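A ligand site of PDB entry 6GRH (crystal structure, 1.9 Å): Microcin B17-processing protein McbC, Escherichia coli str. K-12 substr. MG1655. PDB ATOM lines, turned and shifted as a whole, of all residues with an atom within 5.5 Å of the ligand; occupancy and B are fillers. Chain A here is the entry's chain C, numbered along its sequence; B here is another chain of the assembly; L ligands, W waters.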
ATOM      1  N   ASN A  57      23.090   7.833  21.391  1.00  0.00           N
ATOM      2  CA  ASN A  57      22.946   7.001  20.184  1.00  0.00           C
ATOM      3  C   ASN A  57      23.591   5.632  20.346  1.00  0.00           C
ATOM      4  O   ASN A  57      24.427   5.229  19.535  1.00  0.00           O
ATOM      5  CB  ASN A  57      23.525   7.707  18.949  1.00  0.00           C
ATOM      6  CG  ASN A  57      22.810   9.018  18.664  1.00  0.00           C
ATOM      7  OD1 ASN A  57      21.586   9.062  18.547  1.00  0.00           O
ATOM      8  ND2 ASN A  57      23.578  10.068  18.557  1.00  0.00           N
ATOM      9  N   ARG A  82      15.373  11.145   8.126  1.00  0.00           N
ATOM     10  CA  ARG A  82      14.800  12.263   8.859  1.00  0.00           C
ATOM     11  C   ARG A  82      15.870  13.350   8.877  1.00  0.00           C
ATOM     12  O   ARG A  82      17.040  13.042   9.141  1.00  0.00           O
ATOM     13  CB  ARG A  82      14.437  11.868  10.284  1.00  0.00           C
ATOM     14  CG  ARG A  82      13.916  13.002  11.150  1.00  0.00           C
ATOM     15  CD  ARG A  82      13.485  12.510  12.502  1.00  0.00           C
ATOM     16  NE  ARG A  82      14.559  11.885  13.273  1.00  0.00           N
ATOM     17  CZ  ARG A  82      15.381  12.513  14.091  1.00  0.00           C
ATOM     18  NH1 ARG A  82      15.297  13.832  14.285  1.00  0.00           N
ATOM     19  NH2 ARG A  82      16.317  11.815  14.726  1.00  0.00           N
ATOM     20  N   LEU A  83      15.473  14.589   8.606  1.00  0.00           N
ATOM     21  CA  LEU A  83      16.428  15.716   8.629  1.00  0.00           C
ATOM     22  C   LEU A  83      16.935  15.949  10.063  1.00  0.00           C
ATOM     23  O   LEU A  83      16.178  15.718  11.020  1.00  0.00           O
ATOM     24  CB  LEU A  83      15.776  17.012   8.116  1.00  0.00           C
ATOM     25  CG  LEU A  83      15.302  17.003   6.653  1.00  0.00           C
ATOM     26  CD1 LEU A  83      14.434  18.231   6.381  1.00  0.00           C
ATOM     27  CD2 LEU A  83      16.464  16.978   5.686  1.00  0.00           C
ATOM     28  N   PRO A  84      18.213  16.432  10.202  1.00  0.00           N
ATOM     29  CA  PRO A  84      18.676  16.871  11.524  1.00  0.00           C
ATOM     30  C   PRO A  84      17.706  17.894  12.108  1.00  0.00           C
ATOM     31  O   PRO A  84      17.111  18.671  11.349  1.00  0.00           O
ATOM     32  CB  PRO A  84      20.043  17.490  11.226  1.00  0.00           C
ATOM     33  CG  PRO A  84      20.509  16.841   9.967  1.00  0.00           C
ATOM     34  CD  PRO A  84      19.276  16.539   9.180  1.00  0.00           C
ATOM     35  N   SER A  85      17.471  17.821  13.429  1.00  0.00           N
ATOM     36  CA  SER A  85      16.602  18.793  14.088  1.00  0.00           C
ATOM     37  C   SER A  85      17.202  20.179  13.934  1.00  0.00           C
ATOM     38  O   SER A  85      18.420  20.326  14.030  1.00  0.00           O
ATOM     39  CB  SER A  85      16.423  18.454  15.572  1.00  0.00           C
ATOM     40  OG  SER A  85      15.708  17.228  15.741  1.00  0.00           O
ATOM     41  N   ILE A  87      18.373  24.038  14.583  1.00  0.00           N
ATOM     42  CA  ILE A  87      18.973  24.739  15.721  1.00  0.00           C
ATOM     43  C   ILE A  87      19.583  25.994  15.137  1.00  0.00           C
ATOM     44  O   ILE A  87      19.837  26.039  13.917  1.00  0.00           O
ATOM     45  CB  ILE A  87      20.002  23.829  16.471  1.00  0.00           C
ATOM     46  CG1 ILE A  87      20.316  24.326  17.886  1.00  0.00           C
ATOM     47  CG2 ILE A  87      21.288  23.676  15.669  1.00  0.00           C
ATOM     48  CD1 ILE A  87      19.154  24.340  18.863  1.00  0.00           C
ATOM     49  N   ASP A 178      17.939  28.215  27.221  1.00  0.00           N
ATOM     50  CA  ASP A 178      18.837  27.966  26.071  1.00  0.00           C
ATOM     51  C   ASP A 178      18.445  28.748  24.811  1.00  0.00           C
ATOM     52  O   ASP A 178      18.648  28.288  23.679  1.00  0.00           O
ATOM     53  CB  ASP A 178      18.842  26.449  25.793  1.00  0.00           C
ATOM     54  CG  ASP A 178      20.142  25.946  25.123  1.00  0.00           C
ATOM     55  OD1 ASP A 178      21.214  26.602  25.262  1.00  0.00           O
ATOM     56  OD2 ASP A 178      20.065  24.862  24.491  1.00  0.00           O
ATOM     57  N   ARG A 181      21.155  29.630  21.911  1.00  0.00           N
ATOM     58  CA  ARG A 181      21.455  28.497  21.036  1.00  0.00           C
ATOM     59  C   ARG A 181      20.267  28.198  20.111  1.00  0.00           C
ATOM     60  O   ARG A 181      20.450  27.876  18.938  1.00  0.00           O
ATOM     61  CB  ARG A 181      21.854  27.272  21.877  1.00  0.00           C
ATOM     62  CG  ARG A 181      21.852  25.953  21.148  1.00  0.00           C
ATOM     63  CD  ARG A 181      22.577  24.845  21.904  1.00  0.00           C
ATOM     64  NE  ARG A 181      22.265  23.590  21.240  1.00  0.00           N
ATOM     65  CZ  ARG A 181      21.142  22.901  21.410  1.00  0.00           C
ATOM     66  NH1 ARG A 181      20.204  23.296  22.267  1.00  0.00           N
ATOM     67  NH2 ARG A 181      20.950  21.796  20.692  1.00  0.00           N
ATOM     68  N   TYR A 218       3.560  14.797  17.706  1.00  0.00           N
ATOM     69  CA  TYR A 218       4.719  15.568  17.258  1.00  0.00           C
ATOM     70  C   TYR A 218       5.507  14.828  16.164  1.00  0.00           C
ATOM     71  O   TYR A 218       6.163  15.463  15.343  1.00  0.00           O
ATOM     72  CB  TYR A 218       5.597  16.072  18.399  1.00  0.00           C
ATOM     73  CG  TYR A 218       6.452  15.087  19.171  1.00  0.00           C
ATOM     74  CD1 TYR A 218       7.422  14.305  18.566  1.00  0.00           C
ATOM     75  CD2 TYR A 218       6.343  15.015  20.567  1.00  0.00           C
ATOM     76  CE1 TYR A 218       8.216  13.444  19.315  1.00  0.00           C
ATOM     77  CE2 TYR A 218       7.136  14.164  21.326  1.00  0.00           C
ATOM     78  CZ  TYR A 218       8.076  13.390  20.710  1.00  0.00           C
ATOM     79  OH  TYR A 218       8.840  12.527  21.457  1.00  0.00           O
ATOM     80  N   ARG A 233      12.409  21.349  15.863  1.00  0.00           N
ATOM     81  CA  ARG A 233      13.042  20.727  17.024  1.00  0.00           C
ATOM     82  C   ARG A 233      12.029  20.575  18.159  1.00  0.00           C
ATOM     83  O   ARG A 233      11.441  21.540  18.611  1.00  0.00           O
ATOM     84  CB  ARG A 233      14.244  21.557  17.509  1.00  0.00           C
ATOM     85  CG  ARG A 233      15.001  20.907  18.666  1.00  0.00           C
ATOM     86  CD  ARG A 233      16.311  21.605  19.016  1.00  0.00           C
ATOM     87  NE  ARG A 233      17.357  21.299  18.034  1.00  0.00           N
ATOM     88  CZ  ARG A 233      18.334  20.401  18.160  1.00  0.00           C
ATOM     89  NH1 ARG A 233      18.478  19.666  19.259  1.00  0.00           N
ATOM     90  NH2 ARG A 233      19.171  20.207  17.148  1.00  0.00           N
ATOM     91  N   VAL A 234      11.883  19.341  18.635  1.00  0.00           N
ATOM     92  CA  VAL A 234      11.110  19.049  19.841  1.00  0.00           C
ATOM     93  C   VAL A 234      11.947  19.540  21.010  1.00  0.00           C
ATOM     94  O   VAL A 234      13.155  19.414  20.996  1.00  0.00           O
ATOM     95  CB  VAL A 234      10.745  17.532  19.946  1.00  0.00           C
ATOM     96  CG1 VAL A 234       9.848  17.260  21.156  1.00  0.00           C
ATOM     97  CG2 VAL A 234      10.028  17.072  18.702  1.00  0.00           C
ATOM     98  N   TRP A 235      11.300  20.081  22.030  1.00  0.00           N
ATOM     99  CA  TRP A 235      11.990  20.869  23.022  1.00  0.00           C
ATOM    100  C   TRP A 235      11.327  20.719  24.393  1.00  0.00           C
ATOM    101  O   TRP A 235      10.158  21.010  24.569  1.00  0.00           O
ATOM    102  CB  TRP A 235      11.916  22.306  22.556  1.00  0.00           C
ATOM    103  CG  TRP A 235      12.668  23.299  23.340  1.00  0.00           C
ATOM    104  CD1 TRP A 235      12.190  24.106  24.338  1.00  0.00           C
ATOM    105  CD2 TRP A 235      14.001  23.695  23.101  1.00  0.00           C
ATOM    106  NE1 TRP A 235      13.171  24.966  24.753  1.00  0.00           N
ATOM    107  CE2 TRP A 235      14.299  24.749  24.004  1.00  0.00           C
ATOM    108  CE3 TRP A 235      14.994  23.274  22.196  1.00  0.00           C
ATOM    109  CZ2 TRP A 235      15.531  25.349  24.050  1.00  0.00           C
ATOM    110  CZ3 TRP A 235      16.215  23.882  22.242  1.00  0.00           C
ATOM    111  CH2 TRP A 235      16.484  24.915  23.164  1.00  0.00           C
ATOM    112  N   ALA A 236      12.132  20.312  25.362  1.00  0.00           N
ATOM    113  CA  ALA A 236      11.710  20.153  26.754  1.00  0.00           C
ATOM    114  C   ALA A 236      12.277  21.211  27.700  1.00  0.00           C
ATOM    115  O   ALA A 236      11.921  21.226  28.865  1.00  0.00           O
ATOM    116  CB  ALA A 236      12.102  18.754  27.215  1.00  0.00           C
ATOM    117  N   GLY A 237      13.106  22.113  27.196  1.00  0.00           N
ATOM    118  CA  GLY A 237      13.806  23.082  28.048  1.00  0.00           C
ATOM    119  C   GLY A 237      13.003  24.368  28.219  1.00  0.00           C
ATOM    120  O   GLY A 237      13.404  25.425  27.756  1.00  0.00           O
ATOM    121  N   ILE A 258       5.102  19.263  25.940  1.00  0.00           N
ATOM    122  CA  ILE A 258       6.248  19.377  25.061  1.00  0.00           C
ATOM    123  C   ILE A 258       6.000  20.535  24.107  1.00  0.00           C
ATOM    124  O   ILE A 258       4.853  20.855  23.754  1.00  0.00           O
ATOM    125  CB  ILE A 258       6.539  18.034  24.336  1.00  0.00           C
ATOM    126  CG1 ILE A 258       7.957  17.953  23.821  1.00  0.00           C
ATOM    127  CG2 ILE A 258       5.550  17.751  23.230  1.00  0.00           C
ATOM    128  CD1 ILE A 258       9.002  17.839  24.911  1.00  0.00           C
ATOM    129  N   ARG B 117      21.723   7.961  13.299  1.00  0.00           N
ATOM    130  CA  ARG B 117      20.494   8.718  13.452  1.00  0.00           C
ATOM    131  C   ARG B 117      19.312   7.771  13.208  1.00  0.00           C
ATOM    132  O   ARG B 117      19.462   6.737  12.566  1.00  0.00           O
ATOM    133  CB  ARG B 117      20.521   9.930  12.530  1.00  0.00           C
ATOM    134  CG  ARG B 117      21.691  10.867  12.863  1.00  0.00           C
ATOM    135  CD  ARG B 117      21.547  12.256  12.264  1.00  0.00           C
ATOM    136  NE  ARG B 117      20.255  12.858  12.564  1.00  0.00           N
ATOM    137  CZ  ARG B 117      19.272  12.949  11.687  1.00  0.00           C
ATOM    138  NH1 ARG B 117      19.439  12.485  10.464  1.00  0.00           N
ATOM    139  NH2 ARG B 117      18.124  13.493  12.024  1.00  0.00           N
ATOM    140  N   ARG B 118      18.181   8.068  13.846  1.00  0.00           N
ATOM    141  CA  ARG B 118      16.950   7.307  13.670  1.00  0.00           C
ATOM    142  C   ARG B 118      15.843   8.192  13.107  1.00  0.00           C
ATOM    143  O   ARG B 118      15.923   9.414  13.209  1.00  0.00           O
ATOM    144  CB  ARG B 118      16.515   6.745  15.012  1.00  0.00           C
ATOM    145  CG  ARG B 118      17.589   5.938  15.694  1.00  0.00           C
ATOM    146  CD  ARG B 118      17.037   5.265  16.941  1.00  0.00           C
ATOM    147  NE  ARG B 118      18.118   4.952  17.852  1.00  0.00           N
ATOM    148  CZ  ARG B 118      18.041   4.128  18.891  1.00  0.00           C
ATOM    149  NH1 ARG B 118      16.915   3.510  19.210  1.00  0.00           N
ATOM    150  NH2 ARG B 118      19.139   3.946  19.623  1.00  0.00           N
ATOM    151  N   PRO B 121      13.110  11.417  16.821  1.00  0.00           N
ATOM    152  CA  PRO B 121      14.035  12.075  17.733  1.00  0.00           C
ATOM    153  C   PRO B 121      13.939  11.512  19.151  1.00  0.00           C
ATOM    154  O   PRO B 121      13.060  10.714  19.462  1.00  0.00           O
ATOM    155  CB  PRO B 121      13.579  13.540  17.670  1.00  0.00           C
ATOM    156  CG  PRO B 121      12.089  13.420  17.521  1.00  0.00           C
ATOM    157  CD  PRO B 121      11.844  12.170  16.691  1.00  0.00           C
ATOM    158  N   SER B 122      14.857  11.928  20.024  1.00  0.00           N
ATOM    159  CA  SER B 122      14.839  11.502  21.435  1.00  0.00           C
ATOM    160  C   SER B 122      15.564  12.534  22.288  1.00  0.00           C
ATOM    161  O   SER B 122      16.635  13.016  21.906  1.00  0.00           O
ATOM    162  CB  SER B 122      15.515  10.126  21.589  1.00  0.00           C
ATOM    163  OG  SER B 122      15.607   9.740  22.945  1.00  0.00           O
ATOM    164  N   GLY B 123      14.980  12.860  23.442  1.00  0.00           N
ATOM    165  CA  GLY B 123      15.631  13.775  24.382  1.00  0.00           C
ATOM    166  C   GLY B 123      17.042  13.318  24.708  1.00  0.00           C
ATOM    167  O   GLY B 123      17.255  12.174  25.100  1.00  0.00           O
ATOM    168  N   GLY B 124      18.000  14.213  24.480  1.00  0.00           N
ATOM    169  CA  GLY B 124      19.420  13.936  24.707  1.00  0.00           C
ATOM    170  C   GLY B 124      20.027  12.840  23.865  1.00  0.00           C
ATOM    171  O   GLY B 124      21.109  12.363  24.186  1.00  0.00           O
ATOM    172  N   ALA B 125      19.337  12.453  22.783  1.00  0.00           N
ATOM    173  CA  ALA B 125      19.705  11.306  21.971  1.00  0.00           C
ATOM    174  C   ALA B 125      19.930  10.025  22.794  1.00  0.00           C
ATOM    175  O   ALA B 125      20.781   9.194  22.464  1.00  0.00           O
ATOM    176  CB  ALA B 125      20.940  11.640  21.146  1.00  0.00           C
ATOM    177  N   TYR B 127      17.477   7.628  23.645  1.00  0.00           N
ATOM    178  CA  TYR B 127      16.687   6.472  23.139  1.00  0.00           C
ATOM    179  C   TYR B 127      16.433   5.372  24.180  1.00  0.00           C
ATOM    180  O   TYR B 127      16.893   4.217  24.023  1.00  0.00           O
ATOM    181  CB  TYR B 127      17.356   5.922  21.870  1.00  0.00           C
ATOM    182  CG  TYR B 127      17.289   6.924  20.764  1.00  0.00           C
ATOM    183  CD1 TYR B 127      16.127   7.049  20.010  1.00  0.00           C
ATOM    184  CD2 TYR B 127      18.348   7.807  20.531  1.00  0.00           C
ATOM    185  CE1 TYR B 127      16.018   8.018  19.022  1.00  0.00           C
ATOM    186  CE2 TYR B 127      18.262   8.758  19.515  1.00  0.00           C
ATOM    187  CZ  TYR B 127      17.092   8.863  18.760  1.00  0.00           C
ATOM    188  OH  TYR B 127      16.963   9.820  17.792  1.00  0.00           O
ATOM    189  N   MET B 209       9.408  12.265  28.821  1.00  0.00           N
ATOM    190  CA  MET B 209      10.108  12.188  27.522  1.00  0.00           C
ATOM    191  C   MET B 209      10.108  10.759  26.944  1.00  0.00           C
ATOM    192  O   MET B 209       9.889  10.573  25.743  1.00  0.00           O
ATOM    193  CB  MET B 209      11.554  12.736  27.598  1.00  0.00           C
ATOM    194  CG  MET B 209      11.683  14.264  27.782  1.00  0.00           C
ATOM    195  SD  MET B 209      13.352  14.969  27.518  1.00  0.00           S
ATOM    196  CE  MET B 209      13.502  16.114  28.875  1.00  0.00           C
ATOM    197  N   MET B 212       6.532   9.829  25.639  1.00  0.00           N
ATOM    198  CA  MET B 212       6.331  10.497  24.367  1.00  0.00           C
ATOM    199  C   MET B 212       7.104   9.836  23.233  1.00  0.00           C
ATOM    200  O   MET B 212       6.571   9.613  22.147  1.00  0.00           O
ATOM    201  CB  MET B 212       6.616  12.008  24.478  1.00  0.00           C
ATOM    202  CG  MET B 212       5.591  12.697  25.361  1.00  0.00           C
ATOM    203  SD  MET B 212       5.802  14.473  25.488  1.00  0.00           S
ATOM    204  CE  MET B 212       7.413  14.627  26.223  1.00  0.00           C
HETATM  205  N1  LIG L   1      16.932  19.416  21.891  1.00  0.00           N
HETATM  206  C1  LIG L   1      17.389  20.513  22.551  1.00  0.00           C
HETATM  207  O1  LIG L   1      18.343  21.125  22.054  1.00  0.00           O
HETATM  208  N2  LIG L   1      16.856  20.925  23.727  1.00  0.00           N
HETATM  209  C2  LIG L   1      15.819  20.296  24.311  1.00  0.00           C
HETATM  210  O2  LIG L   1      15.323  20.690  25.389  1.00  0.00           O
HETATM  211  C3  LIG L   1      15.262  19.079  23.656  1.00  0.00           C
HETATM  212  N3  LIG L   1      14.224  18.380  24.180  1.00  0.00           N
HETATM  213  C4  LIG L   1      13.736  17.280  23.538  1.00  0.00           C
HETATM  214  C5  LIG L   1      12.664  16.598  24.100  1.00  0.00           C
HETATM  215  C6  LIG L   1      12.129  15.463  23.477  1.00  0.00           C
HETATM  216  C7  LIG L   1      10.977  14.734  24.115  1.00  0.00           C
HETATM  217  C8  LIG L   1      12.701  14.994  22.192  1.00  0.00           C
HETATM  218  C9  LIG L   1      12.124  13.786  21.517  1.00  0.00           C
HETATM  219  C10 LIG L   1      13.774  15.677  21.610  1.00  0.00           C
HETATM  220  C11 LIG L   1      14.319  16.822  22.234  1.00  0.00           C
HETATM  221  N4  LIG L   1      15.417  17.546  21.674  1.00  0.00           N
HETATM  222  C12 LIG L   1      15.899  18.676  22.375  1.00  0.00           C
HETATM  223  C13 LIG L   1      16.041  17.162  20.412  1.00  0.00           C
HETATM  224  C14 LIG L   1      17.050  16.067  20.640  1.00  0.00           C
HETATM  225  O3  LIG L   1      18.187  16.601  21.352  1.00  0.00           O
HETATM  226  C15 LIG L   1      17.439  15.421  19.307  1.00  0.00           C
HETATM  227  O4  LIG L   1      16.309  14.737  18.756  1.00  0.00           O
HETATM  228  C16 LIG L   1      18.605  14.439  19.423  1.00  0.00           C
HETATM  229  O5  LIG L   1      19.769  15.144  19.866  1.00  0.00           O
HETATM  230  C17 LIG L   1      18.957  13.749  18.108  1.00  0.00           C
HETATM  231  O6  LIG L   1      19.258  14.734  17.130  1.00  0.00           O
HETATM  232  P1  LIG L   1      18.441  14.806  15.751  1.00  0.00           P
HETATM  233  O7  LIG L   1      17.004  15.074  16.114  1.00  0.00           O
HETATM  234  O8  LIG L   1      19.084  15.982  15.038  1.00  0.00           O
HETATM  235  O9  LIG L   1      18.726  13.472  15.145  1.00  0.00           O
HETATM  236  O   HOH W   1      18.381  22.982  25.116  1.00  0.00           O
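The backbone NH (N) of Ser 85 is in hydrogen-bond range of an oxygen (O8) of the ligand (2.9 Å).
An oxygen (O7) of the ligand sits at hydrogen-bond distance from the side-chain hydroxyl (OG) of Ser 85, 2.5 Å away.
An oxygen (O7) of the ligand is in salt-bridge range of the guanidinium group (NH1) of Arg 82.
NH1 of Arg 181 sits at hydrogen-bond distance from O1 of the ligand (2.9 Å).
NE of Arg 117 of chain B is in salt-bridge range of O9 of the ligand, 3.1 Å away.
The guanidinium group of Arg 233 sits at hydrogen-bond distance from a nitrogen (N1) of the ligand (3.1 Å).
N of Ala 236 sits at hydrogen-bond distance from N3 of the ligand.
The backbone NH (N) of Gly 237 is in hydrogen-bond range of an oxygen (O2) of the ligand (3.2 Å).
N of Ser 122 of chain B is in hydrogen-bond range of O4 of the ligand, 3.4 Å away.
O of Ser 85 sits at hydrogen-bond distance from NH2 of Arg 233, at 3.2 Å.
O of Arg 82 is in hydrogen-bond range of NH1 of Arg 117 of chain B (2.8 Å).
The backbone carbonyl oxygen of Arg 118 of chain B sits at hydrogen-bond distance from the guanidinium group of Arg 82 (2.8 Å).
The side-chain carboxylate (OD2) of Asp 178 lies within salt-bridge range of the guanidinium group (NH1) of Arg 181, 2.7 Å away.
The backbone carbonyl oxygen (O) of Leu 83 is in hydrogen-bond range of the guanidinium group (NH2) of Arg 117 of chain B (3.1 Å).
O of Gly 237 sits at hydrogen-bond distance from NE1 of Trp 235, 3.0 Å away.
The side-chain hydroxyl of Ser 122 of chain B is in hydrogen-bond range of the backbone NH of Tyr 127 of chain B (2.9 Å).
The backbone carbonyl oxygen (O) of Ala 125 of chain B sits at hydrogen-bond distance from the backbone NH (N) of Asn 57, 2.9 Å away.
The backbone carbonyl oxygen (O) of Val 234 lies close to a nitrogen (N4) of the ligand (3.0 Å).
Residues that only touch the ligand: Pro 121 of chain B (3.2 Å), Gly 123 of chain B (3.4 Å), Trp 235 (3.4 Å), Tyr 218 (3.5 Å), Pro 84 (3.6 Å), Met 209 of chain B (3.8 Å), Ile 258 (3.8 Å), Ala 125 of chain B (3.9 Å) and Gly 124 of chain B (3.9 Å).
Within 4 Å of the ligand: Arg 82, Pro 84, Ser 85, Arg 181, Tyr 218, Arg 233, Val 234, Trp 235, Ala 236, Gly 237, Ile 258, Arg 117 of chain B, Pro 121 of chain B, Ser 122 of chain B, Gly 123 of chain B, Gly 124 of chain B, Ala 125 of chain B and Met 209 of chain B.
Water W1 lies within hydrogen-bond range of OD2 of Asp 178 (2.6 Å), N2 of the ligand (2.9 Å) and NH1 of Arg 181 (3.4 Å).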
